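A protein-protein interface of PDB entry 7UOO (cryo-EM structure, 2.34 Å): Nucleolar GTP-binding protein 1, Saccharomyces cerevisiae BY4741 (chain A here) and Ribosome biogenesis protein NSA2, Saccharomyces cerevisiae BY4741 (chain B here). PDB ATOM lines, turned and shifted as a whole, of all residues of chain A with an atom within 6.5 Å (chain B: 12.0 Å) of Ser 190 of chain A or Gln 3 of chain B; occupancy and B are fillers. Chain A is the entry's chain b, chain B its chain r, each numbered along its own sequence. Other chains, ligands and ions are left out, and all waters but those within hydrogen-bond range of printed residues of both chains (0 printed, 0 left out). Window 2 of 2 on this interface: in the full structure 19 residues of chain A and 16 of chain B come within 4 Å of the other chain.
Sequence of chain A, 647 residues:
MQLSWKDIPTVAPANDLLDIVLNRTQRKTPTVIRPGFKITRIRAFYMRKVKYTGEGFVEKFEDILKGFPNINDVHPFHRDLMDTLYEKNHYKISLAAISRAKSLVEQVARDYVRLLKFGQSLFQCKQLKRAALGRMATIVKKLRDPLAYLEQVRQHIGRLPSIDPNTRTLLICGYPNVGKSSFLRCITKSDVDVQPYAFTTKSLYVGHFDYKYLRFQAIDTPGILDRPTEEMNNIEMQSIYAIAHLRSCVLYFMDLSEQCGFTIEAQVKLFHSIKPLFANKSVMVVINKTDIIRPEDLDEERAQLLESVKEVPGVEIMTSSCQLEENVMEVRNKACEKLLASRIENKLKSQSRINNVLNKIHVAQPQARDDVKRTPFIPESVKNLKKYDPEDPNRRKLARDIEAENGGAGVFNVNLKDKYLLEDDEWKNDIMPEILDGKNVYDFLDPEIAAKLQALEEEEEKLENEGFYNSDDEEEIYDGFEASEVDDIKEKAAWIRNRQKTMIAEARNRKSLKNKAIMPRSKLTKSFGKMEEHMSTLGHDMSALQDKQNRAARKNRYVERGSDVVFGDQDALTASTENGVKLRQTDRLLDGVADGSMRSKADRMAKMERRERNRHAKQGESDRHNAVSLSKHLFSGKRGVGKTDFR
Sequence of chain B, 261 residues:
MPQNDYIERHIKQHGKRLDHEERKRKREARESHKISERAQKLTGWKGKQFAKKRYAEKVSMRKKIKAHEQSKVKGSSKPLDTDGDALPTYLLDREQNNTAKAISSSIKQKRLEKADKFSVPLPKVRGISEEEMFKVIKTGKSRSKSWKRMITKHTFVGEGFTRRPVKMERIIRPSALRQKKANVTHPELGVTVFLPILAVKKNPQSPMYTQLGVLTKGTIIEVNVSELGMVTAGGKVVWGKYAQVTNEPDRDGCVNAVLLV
N of Asn 4 of chain B is in hydrogen-bond range of O of Arg 159 of chain A.
NE2 of Gln 3 of chain B lies within hydrogen-bond range of OG of Ser 190 of chain A, at 3.3 Å.
The guanidinium group (NH2) of Arg 9 of chain B is in salt-bridge range of the side-chain carboxylate (OD2) of Asp 191 of chain A (2.8 Å).
O of Leu 204 of chain A sits at hydrogen-bond distance from ND2 of Asn 4 of chain B, 3.2 Å away.
NH1 of Arg 9 of chain B sits at hydrogen-bond distance from OH of Tyr 205 of chain A (2.8 Å).
The backbone carbonyl oxygen of Val 206 of chain A is in hydrogen-bond range of the side-chain amide nitrogen of Gln 3 of chain B (3.0 Å).
The side-chain hydroxyl (OG1) of Thr 188 of chain A is in hydrogen-bond range of the backbone NH (N) of Ser 190 of chain A (3.4 Å).
The side-chain hydroxyl (OG) of Ser 190 of chain A lies within hydrogen-bond range of the backbone carbonyl oxygen (O) of Val 206 of chain A, at 3.4 Å.
O of Gln 3 of chain B lies within hydrogen-bond range of NH2 of Arg 9 of chain B (2.9 Å).
The side-chain carboxylate of Asp 5 of chain B is in salt-bridge range of the guanidinium group of Arg 9 of chain B, at 3.2 Å.
O of Arg 159 of chain A touches CA of Gln 3 of chain B, at 3.6 Å.
Arg 159 of chain A touches Tyr 6 of chain B (CD to CE2, 3.8 Å).
Pro 161 of chain A touches Gln 3 of chain B.
Gln 3 of chain B touches Tyr 205 of chain A (OE1 to CA, 3.6 Å).
CZ of Tyr 205 of chain A touches ND2 of Asn 4 of chain B (3.2 Å).
Tyr 205 of chain A touches Asp 5 of chain B.
Of the printed residues of chain B, Pro 161 of chain A touches Gln 3 (3.3 Å).
Ser 162 of chain A touches none of the printed residues of chain B.
No residue of chain B comes within 4 Å of Arg 185 of chain A.
No residue of chain B comes within 4 Å of Thr 188 of chain A.
No residue of chain B comes within 4 Å of Lys 189 of chain A.
Of chain B, only Arg 9 (2.8 Å) comes within 4 Å of Asp 191 of chain A.
No residue of chain B comes within 4 Å of Val 192 of chain A.
Of chain B, only Gln 3 (3.6 Å), Asn 4 (3.2 Å), Asp 5 (3.9 Å) and Arg 9 (2.8 Å) come within 4 Å of Tyr 205 of chain A.
No residue of chain B comes within 4 Å of Gly 207 of chain A.
Gln 3 of chain B touches just these residues of chain A: Arg 159, Pro 161, Ser 190, Tyr 205 and Val 206.
Of the printed residues of chain A, Asn 4 of chain B touches Arg 159 (3.0 Å), Leu 204 (3.2 Å) and Tyr 205 (3.2 Å).
Printed residues of chain A within 4 Å of Asp 5 of chain B: Tyr 205.
Glu 8 of chain B touches none of the printed residues of chain A.
The nearest residue of chain B that does not touch Ser 190 of chain A is Arg 9 of chain B (6.6 Å).
The nearest printed residue of chain A that does not touch Arg 9 of chain B is Val 192 of chain A (5.6 Å).
Of the 13 printed residues of chain B, 5 touch a printed residue of chain A.
Printed residues of chain B that touch a printed residue of chain A: Gln 3, Asn 4, Asp 5, Tyr 6 and Arg 9.
Hydrophobic or aromatic side chains of chain B within 4 Å of the printed part of chain A: Tyr 6.
Of the 16 printed residues of chain A, 7 touch a printed residue of chain B.
Hydrophobic or aromatic side chains of chain A that line the printed part of chain B: Pro 161, Tyr 205 and Val 206.
Among the printed residues, 12 pairs touch across the chains.
Among the printed residues, Asp or Glu carboxylates within 4 Å of a Lys or Arg side-chain nitrogen of the other chain: Asp 191 of chain A with Arg 9 of chain B (2.8 Å).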
ATOM      1  N   ARG A 159      12.231   3.560  -5.124  1.00  0.00           N
ATOM      2  CA  ARG A 159      13.312   2.662  -4.746  1.00  0.00           C
ATOM      3  C   ARG A 159      13.165   2.088  -3.343  1.00  0.00           C
ATOM      4  O   ARG A 159      14.051   1.354  -2.901  1.00  0.00           O
ATOM      5  CB  ARG A 159      14.657   3.388  -4.860  1.00  0.00           C
ATOM      6  CG  ARG A 159      14.889   4.054  -6.207  1.00  0.00           C
ATOM      7  CD  ARG A 159      16.304   4.581  -6.334  1.00  0.00           C
ATOM      8  NE  ARG A 159      16.609   5.625  -5.364  1.00  0.00           N
ATOM      9  CZ  ARG A 159      16.591   6.924  -5.629  1.00  0.00           C
ATOM     10  NH1 ARG A 159      16.295   7.381  -6.833  1.00  0.00           N
ATOM     11  NH2 ARG A 159      16.880   7.788  -4.661  1.00  0.00           N
ATOM     12  N   LEU A 160      12.083   2.398  -2.633  1.00  0.00           N
ATOM     13  CA  LEU A 160      11.902   1.857  -1.293  1.00  0.00           C
ATOM     14  C   LEU A 160      11.647   0.352  -1.359  1.00  0.00           C
ATOM     15  O   LEU A 160      10.903  -0.114  -2.227  1.00  0.00           O
ATOM     16  CB  LEU A 160      10.741   2.542  -0.576  1.00  0.00           C
ATOM     17  CG  LEU A 160      10.919   3.997  -0.148  1.00  0.00           C
ATOM     18  CD1 LEU A 160       9.703   4.460   0.632  1.00  0.00           C
ATOM     19  CD2 LEU A 160      12.181   4.162   0.674  1.00  0.00           C
ATOM     20  N   PRO A 161      12.246  -0.427  -0.461  1.00  0.00           N
ATOM     21  CA  PRO A 161      12.010  -1.874  -0.469  1.00  0.00           C
ATOM     22  C   PRO A 161      10.592  -2.216  -0.041  1.00  0.00           C
ATOM     23  O   PRO A 161       9.945  -1.475   0.701  1.00  0.00           O
ATOM     24  CB  PRO A 161      13.036  -2.403   0.538  1.00  0.00           C
ATOM     25  CG  PRO A 161      13.258  -1.263   1.465  1.00  0.00           C
ATOM     26  CD  PRO A 161      13.157  -0.023   0.623  1.00  0.00           C
ATOM     27  N   SER A 162      10.111  -3.358  -0.525  1.00  0.00           N
ATOM     28  CA  SER A 162       8.768  -3.828  -0.206  1.00  0.00           C
ATOM     29  C   SER A 162       8.826  -4.612   1.099  1.00  0.00           C
ATOM     30  O   SER A 162       9.422  -5.692   1.157  1.00  0.00           O
ATOM     31  CB  SER A 162       8.202  -4.682  -1.336  1.00  0.00           C
ATOM     32  OG  SER A 162       8.855  -5.936  -1.412  1.00  0.00           O
ATOM     33  N   LEU A 184      23.185  -9.874   8.035  1.00  0.00           N
ATOM     34  CA  LEU A 184      22.237  -9.895   6.923  1.00  0.00           C
ATOM     35  C   LEU A 184      22.860 -10.521   5.683  1.00  0.00           C
ATOM     36  O   LEU A 184      22.203 -11.292   4.973  1.00  0.00           O
ATOM     37  CB  LEU A 184      21.740  -8.482   6.617  1.00  0.00           C
ATOM     38  CG  LEU A 184      20.619  -8.402   5.576  1.00  0.00           C
ATOM     39  CD1 LEU A 184      19.306  -8.906   6.154  1.00  0.00           C
ATOM     40  CD2 LEU A 184      20.464  -6.996   5.023  1.00  0.00           C
ATOM     41  N   ARG A 185      24.128 -10.206   5.407  1.00  0.00           N
ATOM     42  CA  ARG A 185      24.831 -10.836   4.293  1.00  0.00           C
ATOM     43  C   ARG A 185      24.954 -12.340   4.494  1.00  0.00           C
ATOM     44  O   ARG A 185      24.843 -13.114   3.537  1.00  0.00           O
ATOM     45  CB  ARG A 185      26.219 -10.222   4.126  1.00  0.00           C
ATOM     46  CG  ARG A 185      26.292  -9.021   3.206  1.00  0.00           C
ATOM     47  CD  ARG A 185      27.745  -8.679   2.931  1.00  0.00           C
ATOM     48  NE  ARG A 185      27.906  -7.464   2.143  1.00  0.00           N
ATOM     49  CZ  ARG A 185      29.080  -6.936   1.822  1.00  0.00           C
ATOM     50  NH1 ARG A 185      30.217  -7.496   2.202  1.00  0.00           N
ATOM     51  NH2 ARG A 185      29.115  -5.817   1.103  1.00  0.00           N
ATOM     52  N   THR A 188      21.010 -13.834   4.288  1.00  0.00           N
ATOM     53  CA  THR A 188      20.267 -13.561   3.064  1.00  0.00           C
ATOM     54  C   THR A 188      21.253 -13.317   1.923  1.00  0.00           C
ATOM     55  O   THR A 188      22.463 -13.507   2.069  1.00  0.00           O
ATOM     56  CB  THR A 188      19.327 -12.364   3.239  1.00  0.00           C
ATOM     57  OG1 THR A 188      20.096 -11.163   3.381  1.00  0.00           O
ATOM     58  CG2 THR A 188      18.439 -12.542   4.458  1.00  0.00           C
ATOM     59  N   LYS A 189      20.727 -12.900   0.774  1.00  0.00           N
ATOM     60  CA  LYS A 189      21.555 -12.519  -0.363  1.00  0.00           C
ATOM     61  C   LYS A 189      21.402 -11.038  -0.693  1.00  0.00           C
ATOM     62  O   LYS A 189      21.591 -10.625  -1.837  1.00  0.00           O
ATOM     63  CB  LYS A 189      21.242 -13.381  -1.585  1.00  0.00           C
ATOM     64  CG  LYS A 189      19.793 -13.379  -2.005  1.00  0.00           C
ATOM     65  CD  LYS A 189      19.610 -14.175  -3.284  1.00  0.00           C
ATOM     66  CE  LYS A 189      20.043 -15.617  -3.108  1.00  0.00           C
ATOM     67  NZ  LYS A 189      19.811 -16.414  -4.343  1.00  0.00           N
ATOM     68  N   SER A 190      21.059 -10.231   0.307  1.00  0.00           N
ATOM     69  CA  SER A 190      20.986  -8.792   0.127  1.00  0.00           C
ATOM     70  C   SER A 190      22.384  -8.208  -0.066  1.00  0.00           C
ATOM     71  O   SER A 190      23.392  -8.774   0.365  1.00  0.00           O
ATOM     72  CB  SER A 190      20.298  -8.138   1.323  1.00  0.00           C
ATOM     73  OG  SER A 190      20.060  -6.762   1.088  1.00  0.00           O
ATOM     74  N   ASP A 191      22.436  -7.057  -0.734  1.00  0.00           N
ATOM     75  CA  ASP A 191      23.688  -6.394  -1.094  1.00  0.00           C
ATOM     76  C   ASP A 191      24.022  -5.235  -0.161  1.00  0.00           C
ATOM     77  O   ASP A 191      24.570  -4.221  -0.601  1.00  0.00           O
ATOM     78  CB  ASP A 191      23.623  -5.909  -2.536  1.00  0.00           C
ATOM     79  CG  ASP A 191      22.387  -5.076  -2.811  1.00  0.00           C
ATOM     80  OD1 ASP A 191      21.292  -5.480  -2.363  1.00  0.00           O
ATOM     81  OD2 ASP A 191      22.510  -4.020  -3.462  1.00  0.00           O
ATOM     82  N   VAL A 192      23.700  -5.355   1.129  1.00  0.00           N
ATOM     83  CA  VAL A 192      23.955  -4.270   2.070  1.00  0.00           C
ATOM     84  C   VAL A 192      25.458  -4.092   2.258  1.00  0.00           C
ATOM     85  O   VAL A 192      26.232  -5.058   2.209  1.00  0.00           O
ATOM     86  CB  VAL A 192      23.230  -4.544   3.403  1.00  0.00           C
ATOM     87  CG1 VAL A 192      23.823  -5.752   4.117  1.00  0.00           C
ATOM     88  CG2 VAL A 192      23.238  -3.306   4.298  1.00  0.00           C
ATOM     89  N   LEU A 204      16.578   1.333   5.759  1.00  0.00           N
ATOM     90  CA  LEU A 204      16.226  -0.059   6.002  1.00  0.00           C
ATOM     91  C   LEU A 204      16.591  -0.926   4.803  1.00  0.00           C
ATOM     92  O   LEU A 204      16.357  -0.550   3.651  1.00  0.00           O
ATOM     93  CB  LEU A 204      14.733  -0.182   6.300  1.00  0.00           C
ATOM     94  CG  LEU A 204      14.220   0.577   7.524  1.00  0.00           C
ATOM     95  CD1 LEU A 204      12.704   0.535   7.590  1.00  0.00           C
ATOM     96  CD2 LEU A 204      14.827   0.005   8.792  1.00  0.00           C
ATOM     97  N   TYR A 205      17.166  -2.094   5.076  1.00  0.00           N
ATOM     98  CA  TYR A 205      17.504  -3.055   4.035  1.00  0.00           C
ATOM     99  C   TYR A 205      16.808  -4.376   4.326  1.00  0.00           C
ATOM    100  O   TYR A 205      16.699  -4.790   5.482  1.00  0.00           O
ATOM    101  CB  TYR A 205      19.017  -3.260   3.925  1.00  0.00           C
ATOM    102  CG  TYR A 205      19.719  -2.211   3.088  1.00  0.00           C
ATOM    103  CD1 TYR A 205      20.083  -0.989   3.634  1.00  0.00           C
ATOM    104  CD2 TYR A 205      20.021  -2.446   1.753  1.00  0.00           C
ATOM    105  CE1 TYR A 205      20.725  -0.029   2.877  1.00  0.00           C
ATOM    106  CE2 TYR A 205      20.665  -1.493   0.987  1.00  0.00           C
ATOM    107  CZ  TYR A 205      21.012  -0.285   1.556  1.00  0.00           C
ATOM    108  OH  TYR A 205      21.651   0.670   0.802  1.00  0.00           O
ATOM    109  N   VAL A 206      16.327  -5.029   3.273  1.00  0.00           N
ATOM    110  CA  VAL A 206      15.511  -6.227   3.396  1.00  0.00           C
ATOM    111  C   VAL A 206      16.222  -7.385   2.712  1.00  0.00           C
ATOM    112  O   VAL A 206      16.777  -7.228   1.619  1.00  0.00           O
ATOM    113  CB  VAL A 206      14.107  -6.022   2.790  1.00  0.00           C
ATOM    114  CG1 VAL A 206      13.204  -7.208   3.102  1.00  0.00           C
ATOM    115  CG2 VAL A 206      13.494  -4.736   3.303  1.00  0.00           C
ATOM    116  N   GLY A 207      16.223  -8.543   3.376  1.00  0.00           N
ATOM    117  CA  GLY A 207      16.623  -9.783   2.752  1.00  0.00           C
ATOM    118  C   GLY A 207      15.563 -10.843   2.993  1.00  0.00           C
ATOM    119  O   GLY A 207      14.630 -10.645   3.767  1.00  0.00           O
ATOM    120  N   HIS A 208      15.728 -11.981   2.324  1.00  0.00           N
ATOM    121  CA  HIS A 208      14.753 -13.056   2.432  1.00  0.00           C
ATOM    122  C   HIS A 208      15.458 -14.395   2.570  1.00  0.00           C
ATOM    123  O   HIS A 208      16.594 -14.567   2.121  1.00  0.00           O
ATOM    124  CB  HIS A 208      13.815 -13.088   1.223  1.00  0.00           C
ATOM    125  CG  HIS A 208      12.763 -12.027   1.250  1.00  0.00           C
ATOM    126  ND1 HIS A 208      12.975 -10.753   0.770  1.00  0.00           N
ATOM    127  CD2 HIS A 208      11.489 -12.052   1.703  1.00  0.00           C
ATOM    128  CE1 HIS A 208      11.875 -10.039   0.925  1.00  0.00           C
ATOM    129  NE2 HIS A 208      10.959 -10.803   1.490  1.00  0.00           N
ATOM    130  N   PRO B   2      16.146  -4.418  -6.527  1.00  0.00           N
ATOM    131  CA  PRO B   2      17.141  -3.530  -5.932  1.00  0.00           C
ATOM    132  C   PRO B   2      16.473  -2.488  -5.035  1.00  0.00           C
ATOM    133  O   PRO B   2      15.324  -2.121  -5.267  1.00  0.00           O
ATOM    134  CB  PRO B   2      17.799  -2.902  -7.150  1.00  0.00           C
ATOM    135  CG  PRO B   2      16.703  -2.808  -8.122  1.00  0.00           C
ATOM    136  CD  PRO B   2      15.808  -4.001  -7.895  1.00  0.00           C
ATOM    137  N   GLN B   3      17.178  -2.033  -4.008  1.00  0.00           N
ATOM    138  CA  GLN B   3      16.595  -1.154  -3.009  1.00  0.00           C
ATOM    139  C   GLN B   3      17.542  -0.004  -2.711  1.00  0.00           C
ATOM    140  O   GLN B   3      18.760  -0.128  -2.861  1.00  0.00           O
ATOM    141  CB  GLN B   3      16.274  -1.926  -1.721  1.00  0.00           C
ATOM    142  CG  GLN B   3      17.414  -2.801  -1.240  1.00  0.00           C
ATOM    143  CD  GLN B   3      16.997  -3.771  -0.156  1.00  0.00           C
ATOM    144  OE1 GLN B   3      16.165  -3.456   0.691  1.00  0.00           O
ATOM    145  NE2 GLN B   3      17.575  -4.963  -0.179  1.00  0.00           N
ATOM    146  N   ASN B   4      16.956   1.116  -2.300  1.00  0.00           N
ATOM    147  CA  ASN B   4      17.664   2.343  -1.896  1.00  0.00           C
ATOM    148  C   ASN B   4      18.473   2.840  -3.102  1.00  0.00           C
ATOM    149  O   ASN B   4      17.986   2.755  -4.239  1.00  0.00           O
ATOM    150  CB  ASN B   4      18.451   2.066  -0.634  1.00  0.00           C
ATOM    151  CG  ASN B   4      17.573   1.546   0.490  1.00  0.00           C
ATOM    152  OD1 ASN B   4      16.596   2.186   0.875  1.00  0.00           O
ATOM    153  ND2 ASN B   4      17.901   0.369   1.003  1.00  0.00           N
ATOM    154  N   ASP B   5      19.688   3.355  -2.906  1.00  0.00           N
ATOM    155  CA  ASP B   5      20.460   3.962  -3.995  1.00  0.00           C
ATOM    156  C   ASP B   5      21.354   2.912  -4.661  1.00  0.00           C
ATOM    157  O   ASP B   5      22.588   2.943  -4.595  1.00  0.00           O
ATOM    158  CB  ASP B   5      21.267   5.144  -3.475  1.00  0.00           C
ATOM    159  CG  ASP B   5      21.993   4.833  -2.180  1.00  0.00           C
ATOM    160  OD1 ASP B   5      21.804   3.724  -1.639  1.00  0.00           O
ATOM    161  OD2 ASP B   5      22.754   5.699  -1.702  1.00  0.00           O
ATOM    162  N   TYR B   6      20.692   1.980  -5.353  1.00  0.00           N
ATOM    163  CA  TYR B   6      21.394   0.815  -5.882  1.00  0.00           C
ATOM    164  C   TYR B   6      22.267   1.153  -7.085  1.00  0.00           C
ATOM    165  O   TYR B   6      23.300   0.512  -7.285  1.00  0.00           O
ATOM    166  CB  TYR B   6      20.397  -0.292  -6.229  1.00  0.00           C
ATOM    167  CG  TYR B   6      19.216   0.143  -7.064  1.00  0.00           C
ATOM    168  CD1 TYR B   6      19.286   0.155  -8.450  1.00  0.00           C
ATOM    169  CD2 TYR B   6      18.018   0.511  -6.465  1.00  0.00           C
ATOM    170  CE1 TYR B   6      18.206   0.546  -9.215  1.00  0.00           C
ATOM    171  CE2 TYR B   6      16.934   0.898  -7.220  1.00  0.00           C
ATOM    172  CZ  TYR B   6      17.033   0.913  -8.595  1.00  0.00           C
ATOM    173  OH  TYR B   6      15.951   1.302  -9.349  1.00  0.00           O
ATOM    174  N   ILE B   7      21.887   2.146  -7.892  1.00  0.00           N
ATOM    175  CA  ILE B   7      22.730   2.545  -9.018  1.00  0.00           C
ATOM    176  C   ILE B   7      24.027   3.168  -8.517  1.00  0.00           C
ATOM    177  O   ILE B   7      25.112   2.880  -9.038  1.00  0.00           O
ATOM    178  CB  ILE B   7      21.962   3.491  -9.961  1.00  0.00           C
ATOM    179  CG1 ILE B   7      20.922   2.713 -10.770  1.00  0.00           C
ATOM    180  CG2 ILE B   7      22.909   4.219 -10.901  1.00  0.00           C
ATOM    181  CD1 ILE B   7      21.514   1.667 -11.687  1.00  0.00           C
ATOM    182  N   GLU B   8      23.939   4.021  -7.494  1.00  0.00           N
ATOM    183  CA  GLU B   8      25.146   4.587  -6.901  1.00  0.00           C
ATOM    184  C   GLU B   8      26.002   3.514  -6.240  1.00  0.00           C
ATOM    185  O   GLU B   8      27.233   3.553  -6.343  1.00  0.00           O
ATOM    186  CB  GLU B   8      24.779   5.679  -5.900  1.00  0.00           C
ATOM    187  CG  GLU B   8      24.537   7.026  -6.546  1.00  0.00           C
ATOM    188  CD  GLU B   8      24.135   8.087  -5.547  1.00  0.00           C
ATOM    189  OE1 GLU B   8      24.477   7.943  -4.356  1.00  0.00           O
ATOM    190  OE2 GLU B   8      23.467   9.062  -5.954  1.00  0.00           O
ATOM    191  N   ARG B   9      25.376   2.546  -5.563  1.00  0.00           N
ATOM    192  CA  ARG B   9      26.152   1.444  -4.996  1.00  0.00           C
ATOM    193  C   ARG B   9      26.833   0.624  -6.089  1.00  0.00           C
ATOM    194  O   ARG B   9      27.976   0.186  -5.924  1.00  0.00           O
ATOM    195  CB  ARG B   9      25.263   0.553  -4.127  1.00  0.00           C
ATOM    196  CG  ARG B   9      24.728   1.242  -2.883  1.00  0.00           C
ATOM    197  CD  ARG B   9      24.319   0.246  -1.811  1.00  0.00           C
ATOM    198  NE  ARG B   9      23.362  -0.744  -2.291  1.00  0.00           N
ATOM    199  CZ  ARG B   9      22.049  -0.565  -2.331  1.00  0.00           C
ATOM    200  NH1 ARG B   9      21.495   0.575  -1.954  1.00  0.00           N
ATOM    201  NH2 ARG B   9      21.271  -1.555  -2.759  1.00  0.00           N
ATOM    202  N   HIS B  10      26.147   0.410  -7.215  1.00  0.00           N
ATOM    203  CA  HIS B  10      26.745  -0.318  -8.328  1.00  0.00           C
ATOM    204  C   HIS B  10      27.925   0.444  -8.920  1.00  0.00           C
ATOM    205  O   HIS B  10      28.932  -0.158  -9.301  1.00  0.00           O
ATOM    206  CB  HIS B  10      25.693  -0.589  -9.404  1.00  0.00           C
ATOM    207  CG  HIS B  10      26.226  -1.322 -10.595  1.00  0.00           C
ATOM    208  ND1 HIS B  10      26.207  -2.697 -10.692  1.00  0.00           N
ATOM    209  CD2 HIS B  10      26.797  -0.873 -11.737  1.00  0.00           C
ATOM    210  CE1 HIS B  10      26.741  -3.062 -11.844  1.00  0.00           C
ATOM    211  NE2 HIS B  10      27.110  -1.974 -12.495  1.00  0.00           N
ATOM    212  N   ILE B  11      27.804   1.769  -9.028  1.00  0.00           N
ATOM    213  CA  ILE B  11      28.912   2.583  -9.517  1.00  0.00           C
ATOM    214  C   ILE B  11      30.083   2.522  -8.543  1.00  0.00           C
ATOM    215  O   ILE B  11      31.249   2.456  -8.950  1.00  0.00           O
ATOM    216  CB  ILE B  11      28.441   4.029  -9.760  1.00  0.00           C
ATOM    217  CG1 ILE B  11      27.479   4.086 -10.948  1.00  0.00           C
ATOM    218  CG2 ILE B  11      29.618   4.960  -9.991  1.00  0.00           C
ATOM    219  CD1 ILE B  11      26.887   5.458 -11.189  1.00  0.00           C
ATOM    220  N   LYS B  12      29.789   2.520  -7.244  1.00  0.00           N
ATOM    221  CA  LYS B  12      30.835   2.419  -6.233  1.00  0.00           C
ATOM    222  C   LYS B  12      31.526   1.059  -6.259  1.00  0.00           C
ATOM    223  O   LYS B  12      32.724   0.972  -5.972  1.00  0.00           O
ATOM    224  CB  LYS B  12      30.238   2.684  -4.852  1.00  0.00           C
ATOM    225  CG  LYS B  12      31.021   3.663  -4.006  1.00  0.00           C
ATOM    226  CD  LYS B  12      30.228   4.070  -2.779  1.00  0.00           C
ATOM    227  CE  LYS B  12      28.937   4.773  -3.168  1.00  0.00           C
ATOM    228  NZ  LYS B  12      28.090   5.069  -1.985  1.00  0.00           N
ATOM    229  N   GLN B  13      30.795  -0.005  -6.593  1.00  0.00           N
ATOM    230  CA  GLN B  13      31.347  -1.354  -6.524  1.00  0.00           C
ATOM    231  C   GLN B  13      32.007  -1.817  -7.817  1.00  0.00           C
ATOM    232  O   GLN B  13      32.968  -2.591  -7.761  1.00  0.00           O
ATOM    233  CB  GLN B  13      30.254  -2.352  -6.138  1.00  0.00           C
ATOM    234  CG  GLN B  13      29.792  -2.255  -4.695  1.00  0.00           C
ATOM    235  CD  GLN B  13      30.847  -2.710  -3.708  1.00  0.00           C
ATOM    236  OE1 GLN B  13      30.968  -3.900  -3.419  1.00  0.00           O
ATOM    237  NE2 GLN B  13      31.616  -1.764  -3.182  1.00  0.00           N
ATOM    238  N   HIS B  14      31.515  -1.381  -8.977  1.00  0.00           N
ATOM    239  CA  HIS B  14      32.020  -1.850 -10.258  1.00  0.00           C
ATOM    240  C   HIS B  14      32.531  -0.743 -11.169  1.00  0.00           C
ATOM    241  O   HIS B  14      33.088  -1.052 -12.227  1.00  0.00           O
ATOM    242  CB  HIS B  14      30.931  -2.630 -11.013  1.00  0.00           C
ATOM    243  CG  HIS B  14      30.265  -3.691 -10.196  1.00  0.00           C
ATOM    244  ND1 HIS B  14      30.779  -4.962 -10.062  1.00  0.00           N
ATOM    245  CD2 HIS B  14      29.120  -3.671  -9.473  1.00  0.00           C
ATOM    246  CE1 HIS B  14      29.983  -5.677  -9.288  1.00  0.00           C
ATOM    247  NE2 HIS B  14      28.968  -4.917  -8.919  1.00  0.00           N
